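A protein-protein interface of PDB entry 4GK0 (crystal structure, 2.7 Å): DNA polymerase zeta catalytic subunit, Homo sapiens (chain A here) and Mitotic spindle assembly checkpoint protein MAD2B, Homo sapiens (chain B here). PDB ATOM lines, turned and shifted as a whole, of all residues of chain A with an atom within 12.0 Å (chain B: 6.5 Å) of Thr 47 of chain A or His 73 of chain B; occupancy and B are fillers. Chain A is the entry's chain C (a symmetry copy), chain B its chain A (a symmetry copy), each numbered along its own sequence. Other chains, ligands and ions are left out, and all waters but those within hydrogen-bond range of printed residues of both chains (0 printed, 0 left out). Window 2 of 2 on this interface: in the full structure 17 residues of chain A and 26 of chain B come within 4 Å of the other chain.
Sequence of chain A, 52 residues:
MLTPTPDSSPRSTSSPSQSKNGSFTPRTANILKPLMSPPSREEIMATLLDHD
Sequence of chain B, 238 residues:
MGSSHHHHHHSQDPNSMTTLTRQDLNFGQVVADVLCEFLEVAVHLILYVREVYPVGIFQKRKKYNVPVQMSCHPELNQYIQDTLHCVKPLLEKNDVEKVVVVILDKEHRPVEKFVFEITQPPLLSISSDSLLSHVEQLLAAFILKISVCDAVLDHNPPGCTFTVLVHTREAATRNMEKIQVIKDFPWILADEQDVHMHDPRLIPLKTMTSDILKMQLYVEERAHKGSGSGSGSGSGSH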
ATOM      1  N   SER A  37      12.198 -13.487 -16.606  1.00  0.00           N
ATOM      2  CA  SER A  37      11.464 -12.587 -17.464  1.00  0.00           C
ATOM      3  C   SER A  37      11.998 -12.601 -18.868  1.00  0.00           C
ATOM      4  O   SER A  37      13.201 -12.673 -19.054  1.00  0.00           O
ATOM      5  CB  SER A  37      11.642 -11.189 -16.922  1.00  0.00           C
ATOM      6  OG  SER A  37      10.751 -11.015 -15.839  1.00  0.00           O
ATOM      7  N   PRO A  38      11.120 -12.482 -19.868  1.00  0.00           N
ATOM      8  CA  PRO A  38      11.679 -12.194 -21.184  1.00  0.00           C
ATOM      9  C   PRO A  38      12.345 -10.820 -21.222  1.00  0.00           C
ATOM     10  O   PRO A  38      12.011  -9.983 -20.407  1.00  0.00           O
ATOM     11  CB  PRO A  38      10.457 -12.236 -22.103  1.00  0.00           C
ATOM     12  CG  PRO A  38       9.345 -11.842 -21.246  1.00  0.00           C
ATOM     13  CD  PRO A  38       9.664 -12.283 -19.838  1.00  0.00           C
ATOM     14  N   PRO A  39      13.288 -10.590 -22.162  1.00  0.00           N
ATOM     15  CA  PRO A  39      13.848  -9.251 -22.325  1.00  0.00           C
ATOM     16  C   PRO A  39      12.764  -8.213 -22.540  1.00  0.00           C
ATOM     17  O   PRO A  39      11.873  -8.415 -23.374  1.00  0.00           O
ATOM     18  CB  PRO A  39      14.686  -9.362 -23.580  1.00  0.00           C
ATOM     19  CG  PRO A  39      14.242 -10.593 -24.267  1.00  0.00           C
ATOM     20  CD  PRO A  39      13.807 -11.516 -23.176  1.00  0.00           C
ATOM     21  N   SER A  40      12.838  -7.120 -21.779  1.00  0.00           N
ATOM     22  CA  SER A  40      11.830  -6.051 -21.851  1.00  0.00           C
ATOM     23  C   SER A  40      11.879  -5.296 -23.181  1.00  0.00           C
ATOM     24  O   SER A  40      12.756  -5.545 -24.026  1.00  0.00           O
ATOM     25  CB  SER A  40      12.025  -5.049 -20.704  1.00  0.00           C
ATOM     26  OG  SER A  40      13.172  -4.237 -20.909  1.00  0.00           O
ATOM     27  N   ARG A  41      10.924  -4.386 -23.347  1.00  0.00           N
ATOM     28  CA  ARG A  41      10.875  -3.485 -24.519  1.00  0.00           C
ATOM     29  C   ARG A  41      12.123  -2.597 -24.560  1.00  0.00           C
ATOM     30  O   ARG A  41      12.847  -2.607 -25.549  1.00  0.00           O
ATOM     31  CB  ARG A  41       9.582  -2.653 -24.518  1.00  0.00           C
ATOM     32  CG  ARG A  41       9.033  -2.321 -25.891  1.00  0.00           C
ATOM     33  CD  ARG A  41       7.588  -1.830 -25.812  1.00  0.00           C
ATOM     34  NE  ARG A  41       7.330  -0.762 -26.780  1.00  0.00           N
ATOM     35  CZ  ARG A  41       6.725  -0.892 -27.963  1.00  0.00           C
ATOM     36  NH1 ARG A  41       6.250  -2.061 -28.384  1.00  0.00           N
ATOM     37  NH2 ARG A  41       6.586   0.176 -28.746  1.00  0.00           N
ATOM     38  N   GLU A  42      12.382  -1.883 -23.466  1.00  0.00           N
ATOM     39  CA  GLU A  42      13.643  -1.143 -23.252  1.00  0.00           C
ATOM     40  C   GLU A  42      14.864  -1.919 -23.731  1.00  0.00           C
ATOM     41  O   GLU A  42      15.533  -1.508 -24.654  1.00  0.00           O
ATOM     42  CB  GLU A  42      13.873  -0.804 -21.761  1.00  0.00           C
ATOM     43  CG  GLU A  42      12.790   0.015 -21.068  1.00  0.00           C
ATOM     44  CD  GLU A  42      11.649  -0.842 -20.510  1.00  0.00           C
ATOM     45  OE1 GLU A  42      11.200  -1.761 -21.238  1.00  0.00           O
ATOM     46  OE2 GLU A  42      11.189  -0.600 -19.361  1.00  0.00           O
ATOM     47  N   GLU A  43      15.128  -3.052 -23.094  1.00  0.00           N
ATOM     48  CA  GLU A  43      16.317  -3.878 -23.339  1.00  0.00           C
ATOM     49  C   GLU A  43      16.475  -4.207 -24.814  1.00  0.00           C
ATOM     50  O   GLU A  43      17.523  -4.666 -25.241  1.00  0.00           O
ATOM     51  CB  GLU A  43      16.190  -5.187 -22.548  1.00  0.00           C
ATOM     52  CG  GLU A  43      17.479  -5.854 -22.064  1.00  0.00           C
ATOM     53  CD  GLU A  43      17.240  -6.785 -20.856  1.00  0.00           C
ATOM     54  OE1 GLU A  43      16.073  -6.869 -20.370  1.00  0.00           O
ATOM     55  OE2 GLU A  43      18.212  -7.440 -20.379  1.00  0.00           O
ATOM     56  N   ILE A  44      15.417  -3.994 -25.586  1.00  0.00           N
ATOM     57  CA  ILE A  44      15.416  -4.314 -27.007  1.00  0.00           C
ATOM     58  C   ILE A  44      15.740  -3.076 -27.823  1.00  0.00           C
ATOM     59  O   ILE A  44      16.425  -3.173 -28.853  1.00  0.00           O
ATOM     60  CB  ILE A  44      14.048  -4.881 -27.460  1.00  0.00           C
ATOM     61  CG1 ILE A  44      13.844  -6.306 -26.923  1.00  0.00           C
ATOM     62  CG2 ILE A  44      13.929  -4.855 -28.982  1.00  0.00           C
ATOM     63  CD1 ILE A  44      14.160  -7.399 -27.919  1.00  0.00           C
ATOM     64  N   MET A  45      15.269  -1.921 -27.353  1.00  0.00           N
ATOM     65  CA  MET A  45      15.395  -0.668 -28.109  1.00  0.00           C
ATOM     66  C   MET A  45      16.806  -0.464 -28.690  1.00  0.00           C
ATOM     67  O   MET A  45      16.987   0.309 -29.632  1.00  0.00           O
ATOM     68  CB  MET A  45      14.995   0.536 -27.240  1.00  0.00           C
ATOM     69  CG  MET A  45      16.120   1.126 -26.399  1.00  0.00           C
ATOM     70  SD  MET A  45      15.469   2.075 -25.005  1.00  0.00           S
ATOM     71  CE  MET A  45      16.770   1.791 -23.776  1.00  0.00           C
ATOM     72  N   ALA A  46      17.789  -1.174 -28.136  1.00  0.00           N
ATOM     73  CA  ALA A  46      19.168  -1.049 -28.567  1.00  0.00           C
ATOM     74  C   ALA A  46      19.825  -2.413 -28.833  1.00  0.00           C
ATOM     75  O   ALA A  46      20.603  -2.903 -28.011  1.00  0.00           O
ATOM     76  CB  ALA A  46      19.955  -0.254 -27.525  1.00  0.00           C
ATOM     77  N   THR A  47      19.501  -3.023 -29.976  1.00  0.00           N
ATOM     78  CA  THR A  47      20.286  -4.160 -30.521  1.00  0.00           C
ATOM     79  C   THR A  47      20.000  -4.399 -32.005  1.00  0.00           C
ATOM     80  O   THR A  47      18.905  -4.107 -32.487  1.00  0.00           O
ATOM     81  CB  THR A  47      20.030  -5.478 -29.760  1.00  0.00           C
ATOM     82  OG1 THR A  47      18.839  -5.343 -28.965  1.00  0.00           O
ATOM     83  CG2 THR A  47      21.224  -5.844 -28.862  1.00  0.00           C
ATOM     84  N   HIS B  44       5.236 -15.718 -31.303  1.00  0.00           N
ATOM     85  CA  HIS B  44       5.884 -14.601 -31.997  1.00  0.00           C
ATOM     86  C   HIS B  44       4.798 -13.700 -32.563  1.00  0.00           C
ATOM     87  O   HIS B  44       4.788 -12.510 -32.335  1.00  0.00           O
ATOM     88  CB  HIS B  44       6.748 -15.109 -33.133  1.00  0.00           C
ATOM     89  CG  HIS B  44       8.125 -15.495 -32.720  1.00  0.00           C
ATOM     90  ND1 HIS B  44       9.141 -14.583 -32.585  1.00  0.00           N
ATOM     91  CD2 HIS B  44       8.673 -16.698 -32.463  1.00  0.00           C
ATOM     92  CE1 HIS B  44      10.250 -15.200 -32.237  1.00  0.00           C
ATOM     93  NE2 HIS B  44       9.991 -16.487 -32.161  1.00  0.00           N
ATOM     94  N   ILE B  57      11.434  -5.149 -34.845  1.00  0.00           N
ATOM     95  CA  ILE B  57      12.193  -6.379 -34.601  1.00  0.00           C
ATOM     96  C   ILE B  57      11.706  -7.621 -35.350  1.00  0.00           C
ATOM     97  O   ILE B  57      12.334  -8.678 -35.242  1.00  0.00           O
ATOM     98  CB  ILE B  57      12.292  -6.712 -33.109  1.00  0.00           C
ATOM     99  CG1 ILE B  57      10.921  -7.037 -32.536  1.00  0.00           C
ATOM    100  CG2 ILE B  57      12.915  -5.562 -32.353  1.00  0.00           C
ATOM    101  CD1 ILE B  57      10.990  -7.838 -31.256  1.00  0.00           C
ATOM    102  N   MET B  70       8.075 -13.132 -37.473  1.00  0.00           N
ATOM    103  CA  MET B  70       9.001 -13.713 -36.496  1.00  0.00           C
ATOM    104  C   MET B  70      10.024 -12.683 -36.057  1.00  0.00           C
ATOM    105  O   MET B  70      10.648 -12.020 -36.869  1.00  0.00           O
ATOM    106  CB  MET B  70       9.798 -14.859 -37.089  1.00  0.00           C
ATOM    107  CG  MET B  70       9.012 -15.894 -37.851  1.00  0.00           C
ATOM    108  SD  MET B  70       8.176 -16.975 -36.720  1.00  0.00           S
ATOM    109  CE  MET B  70       9.508 -18.021 -36.123  1.00  0.00           C
ATOM    110  N   SER B  71      10.207 -12.569 -34.757  1.00  0.00           N
ATOM    111  CA  SER B  71      11.227 -11.704 -34.191  1.00  0.00           C
ATOM    112  C   SER B  71      12.633 -12.104 -34.655  1.00  0.00           C
ATOM    113  O   SER B  71      12.924 -13.282 -34.879  1.00  0.00           O
ATOM    114  CB  SER B  71      11.140 -11.711 -32.664  1.00  0.00           C
ATOM    115  OG  SER B  71      12.390 -11.465 -32.060  1.00  0.00           O
ATOM    116  N   CYS B  72      13.470 -11.084 -34.805  1.00  0.00           N
ATOM    117  CA  CYS B  72      14.873 -11.204 -35.216  1.00  0.00           C
ATOM    118  C   CYS B  72      15.834 -11.061 -34.060  1.00  0.00           C
ATOM    119  O   CYS B  72      17.038 -11.213 -34.228  1.00  0.00           O
ATOM    120  CB  CYS B  72      15.218 -10.083 -36.203  1.00  0.00           C
ATOM    121  SG  CYS B  72      14.586 -10.527 -37.813  1.00  0.00           S
ATOM    122  N   HIS B  73      15.298 -10.724 -32.900  1.00  0.00           N
ATOM    123  CA  HIS B  73      16.124 -10.366 -31.807  1.00  0.00           C
ATOM    124  C   HIS B  73      16.574 -11.631 -31.075  1.00  0.00           C
ATOM    125  O   HIS B  73      15.742 -12.342 -30.516  1.00  0.00           O
ATOM    126  CB  HIS B  73      15.392  -9.440 -30.874  1.00  0.00           C
ATOM    127  CG  HIS B  73      16.293  -8.851 -29.850  1.00  0.00           C
ATOM    128  ND1 HIS B  73      16.820  -9.599 -28.820  1.00  0.00           N
ATOM    129  CD2 HIS B  73      16.827  -7.614 -29.735  1.00  0.00           C
ATOM    130  CE1 HIS B  73      17.610  -8.836 -28.089  1.00  0.00           C
ATOM    131  NE2 HIS B  73      17.627  -7.626 -28.619  1.00  0.00           N
ATOM    132  N   PRO B  74      17.897 -11.907 -31.073  1.00  0.00           N
ATOM    133  CA  PRO B  74      18.464 -13.168 -30.595  1.00  0.00           C
ATOM    134  C   PRO B  74      18.161 -13.540 -29.134  1.00  0.00           C
ATOM    135  O   PRO B  74      17.914 -14.698 -28.857  1.00  0.00           O
ATOM    136  CB  PRO B  74      19.972 -12.958 -30.812  1.00  0.00           C
ATOM    137  CG  PRO B  74      20.056 -11.997 -31.928  1.00  0.00           C
ATOM    138  CD  PRO B  74      18.966 -11.025 -31.581  1.00  0.00           C
ATOM    139  N   GLU B  75      18.170 -12.575 -28.221  1.00  0.00           N
ATOM    140  CA  GLU B  75      17.859 -12.824 -26.809  1.00  0.00           C
ATOM    141  C   GLU B  75      16.380 -13.278 -26.677  1.00  0.00           C
ATOM    142  O   GLU B  75      16.088 -14.370 -26.204  1.00  0.00           O
ATOM    143  CB  GLU B  75      18.159 -11.570 -25.956  1.00  0.00           C
ATOM    144  CG  GLU B  75      18.848 -11.839 -24.615  1.00  0.00           C
ATOM    145  CD  GLU B  75      18.477 -10.853 -23.491  1.00  0.00           C
ATOM    146  OE1 GLU B  75      18.632  -9.625 -23.693  1.00  0.00           O
ATOM    147  OE2 GLU B  75      18.040 -11.303 -22.398  1.00  0.00           O
ATOM    148  N   LEU B  76      15.451 -12.442 -27.131  1.00  0.00           N
ATOM    149  CA  LEU B  76      14.049 -12.812 -27.213  1.00  0.00           C
ATOM    150  C   LEU B  76      13.829 -14.142 -27.893  1.00  0.00           C
ATOM    151  O   LEU B  76      13.044 -14.956 -27.412  1.00  0.00           O
ATOM    152  CB  LEU B  76      13.215 -11.750 -27.950  1.00  0.00           C
ATOM    153  CG  LEU B  76      11.717 -12.049 -27.951  1.00  0.00           C
ATOM    154  CD1 LEU B  76      11.176 -11.966 -26.524  1.00  0.00           C
ATOM    155  CD2 LEU B  76      10.921 -11.163 -28.876  1.00  0.00           C
ATOM    156  N   ASN B  77      14.464 -14.370 -29.029  1.00  0.00           N
ATOM    157  CA  ASN B  77      14.245 -15.654 -29.702  1.00  0.00           C
ATOM    158  C   ASN B  77      14.675 -16.832 -28.831  1.00  0.00           C
ATOM    159  O   ASN B  77      14.063 -17.858 -28.833  1.00  0.00           O
ATOM    160  CB  ASN B  77      14.927 -15.714 -31.065  1.00  0.00           C
ATOM    161  CG  ASN B  77      14.321 -14.764 -32.067  1.00  0.00           C
ATOM    162  OD1 ASN B  77      13.495 -13.911 -31.733  1.00  0.00           O
ATOM    163  ND2 ASN B  77      14.730 -14.900 -33.301  1.00  0.00           N
ATOM    164  N   GLN B  78      15.730 -16.640 -28.061  1.00  0.00           N
ATOM    165  CA  GLN B  78      16.310 -17.708 -27.294  1.00  0.00           C
ATOM    166  C   GLN B  78      15.386 -17.980 -26.099  1.00  0.00           C
ATOM    167  O   GLN B  78      15.189 -19.129 -25.702  1.00  0.00           O
ATOM    168  CB  GLN B  78      17.729 -17.309 -26.834  1.00  0.00           C
ATOM    169  CG  GLN B  78      18.511 -18.411 -26.120  1.00  0.00           C
ATOM    170  CD  GLN B  78      18.948 -19.449 -27.108  1.00  0.00           C
ATOM    171  OE1 GLN B  78      19.696 -19.141 -28.028  1.00  0.00           O
ATOM    172  NE2 GLN B  78      18.459 -20.670 -26.961  1.00  0.00           N
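Of the 11 printed residues of chain B, 4 touch a printed residue of chain A.
Hydrophobic or aromatic side chains of chain B within 4 Å of the printed part of chain A: Ile 57, His 73 and Leu 76.
Hydrophobic or aromatic side chains of chain A within 4 Å of the printed part of chain B: Pro 39 and Ile 44.
Among the printed residues, no Asp or Glu carboxylate lies within 4 Å of a Lys or Arg side-chain nitrogen of the other chain.
Of chain B, only His 73 comes within 4 Å of Thr 47 of chain A.
Of chain A, only Ile 44 and Thr 47 come within 4 Å of His 73 of chain B.
Leu 76 of chain B touches just one residue of chain A: Pro 39 (3.6 Å).
No residue of chain A comes within 4 Å of Asn 77 of chain B.
Printed residues of chain B within 4 Å of Glu 43 of chain A: Glu 75.
Printed residues of chain A within 4 Å of Glu 75 of chain B: Pro 39 and Glu 43.
Printed residues of chain B within 4 Å of Pro 39 of chain A: Glu 75 (3.96 Å) and Leu 76 (3.6 Å).
Of the printed residues of chain B, Ile 44 of chain A touches Ile 57 (3.6 Å) and His 73 (3.2 Å).
Glu 42 of chain A touches none of the printed residues of chain B.
His 44 of chain B touches none of the printed residues of chain A.
The side-chain hydroxyl of Thr 47 of chain A sits at hydrogen-bond distance from a ring nitrogen (NE2) of His 73 of chain B.
Among the printed residues, merely in contact across the chains: Pro 39 of chain A with Glu 75 of chain B (3.96 Å), Pro 39 of chain A with Leu 76 of chain B (3.6 Å), Glu 43 of chain A with Glu 75 of chain B (3.99 Å), Ile 44 of chain A with Ile 57 of chain B (3.6 Å) and Ile 44 of chain A with His 73 of chain B (3.2 Å).
The backbone carbonyl oxygen of Ile 57 of chain B is in hydrogen-bond range of the backbone NH of Cys 72 of chain B.
OG of Ser 71 of chain B lies within hydrogen-bond range of N of His 73 of chain B (3.1 Å).
N of Glu 75 of chain B is in hydrogen-bond range of ND1 of His 73 of chain B, 3.3 Å away.
The backbone carbonyl oxygen (O) of His 73 of chain B lies close to the side-chain amide oxygen (OD1) of Asn 77 of chain B (3.0 Å).
The backbone NH (N) of Glu 43 of chain A is in hydrogen-bond range of the side-chain hydroxyl (OG) of Ser 40 of chain A, 3.2 Å away.
OG1 of Thr 47 of chain A sits at hydrogen-bond distance from O of Ile 44 of chain A, at 3.2 Å.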
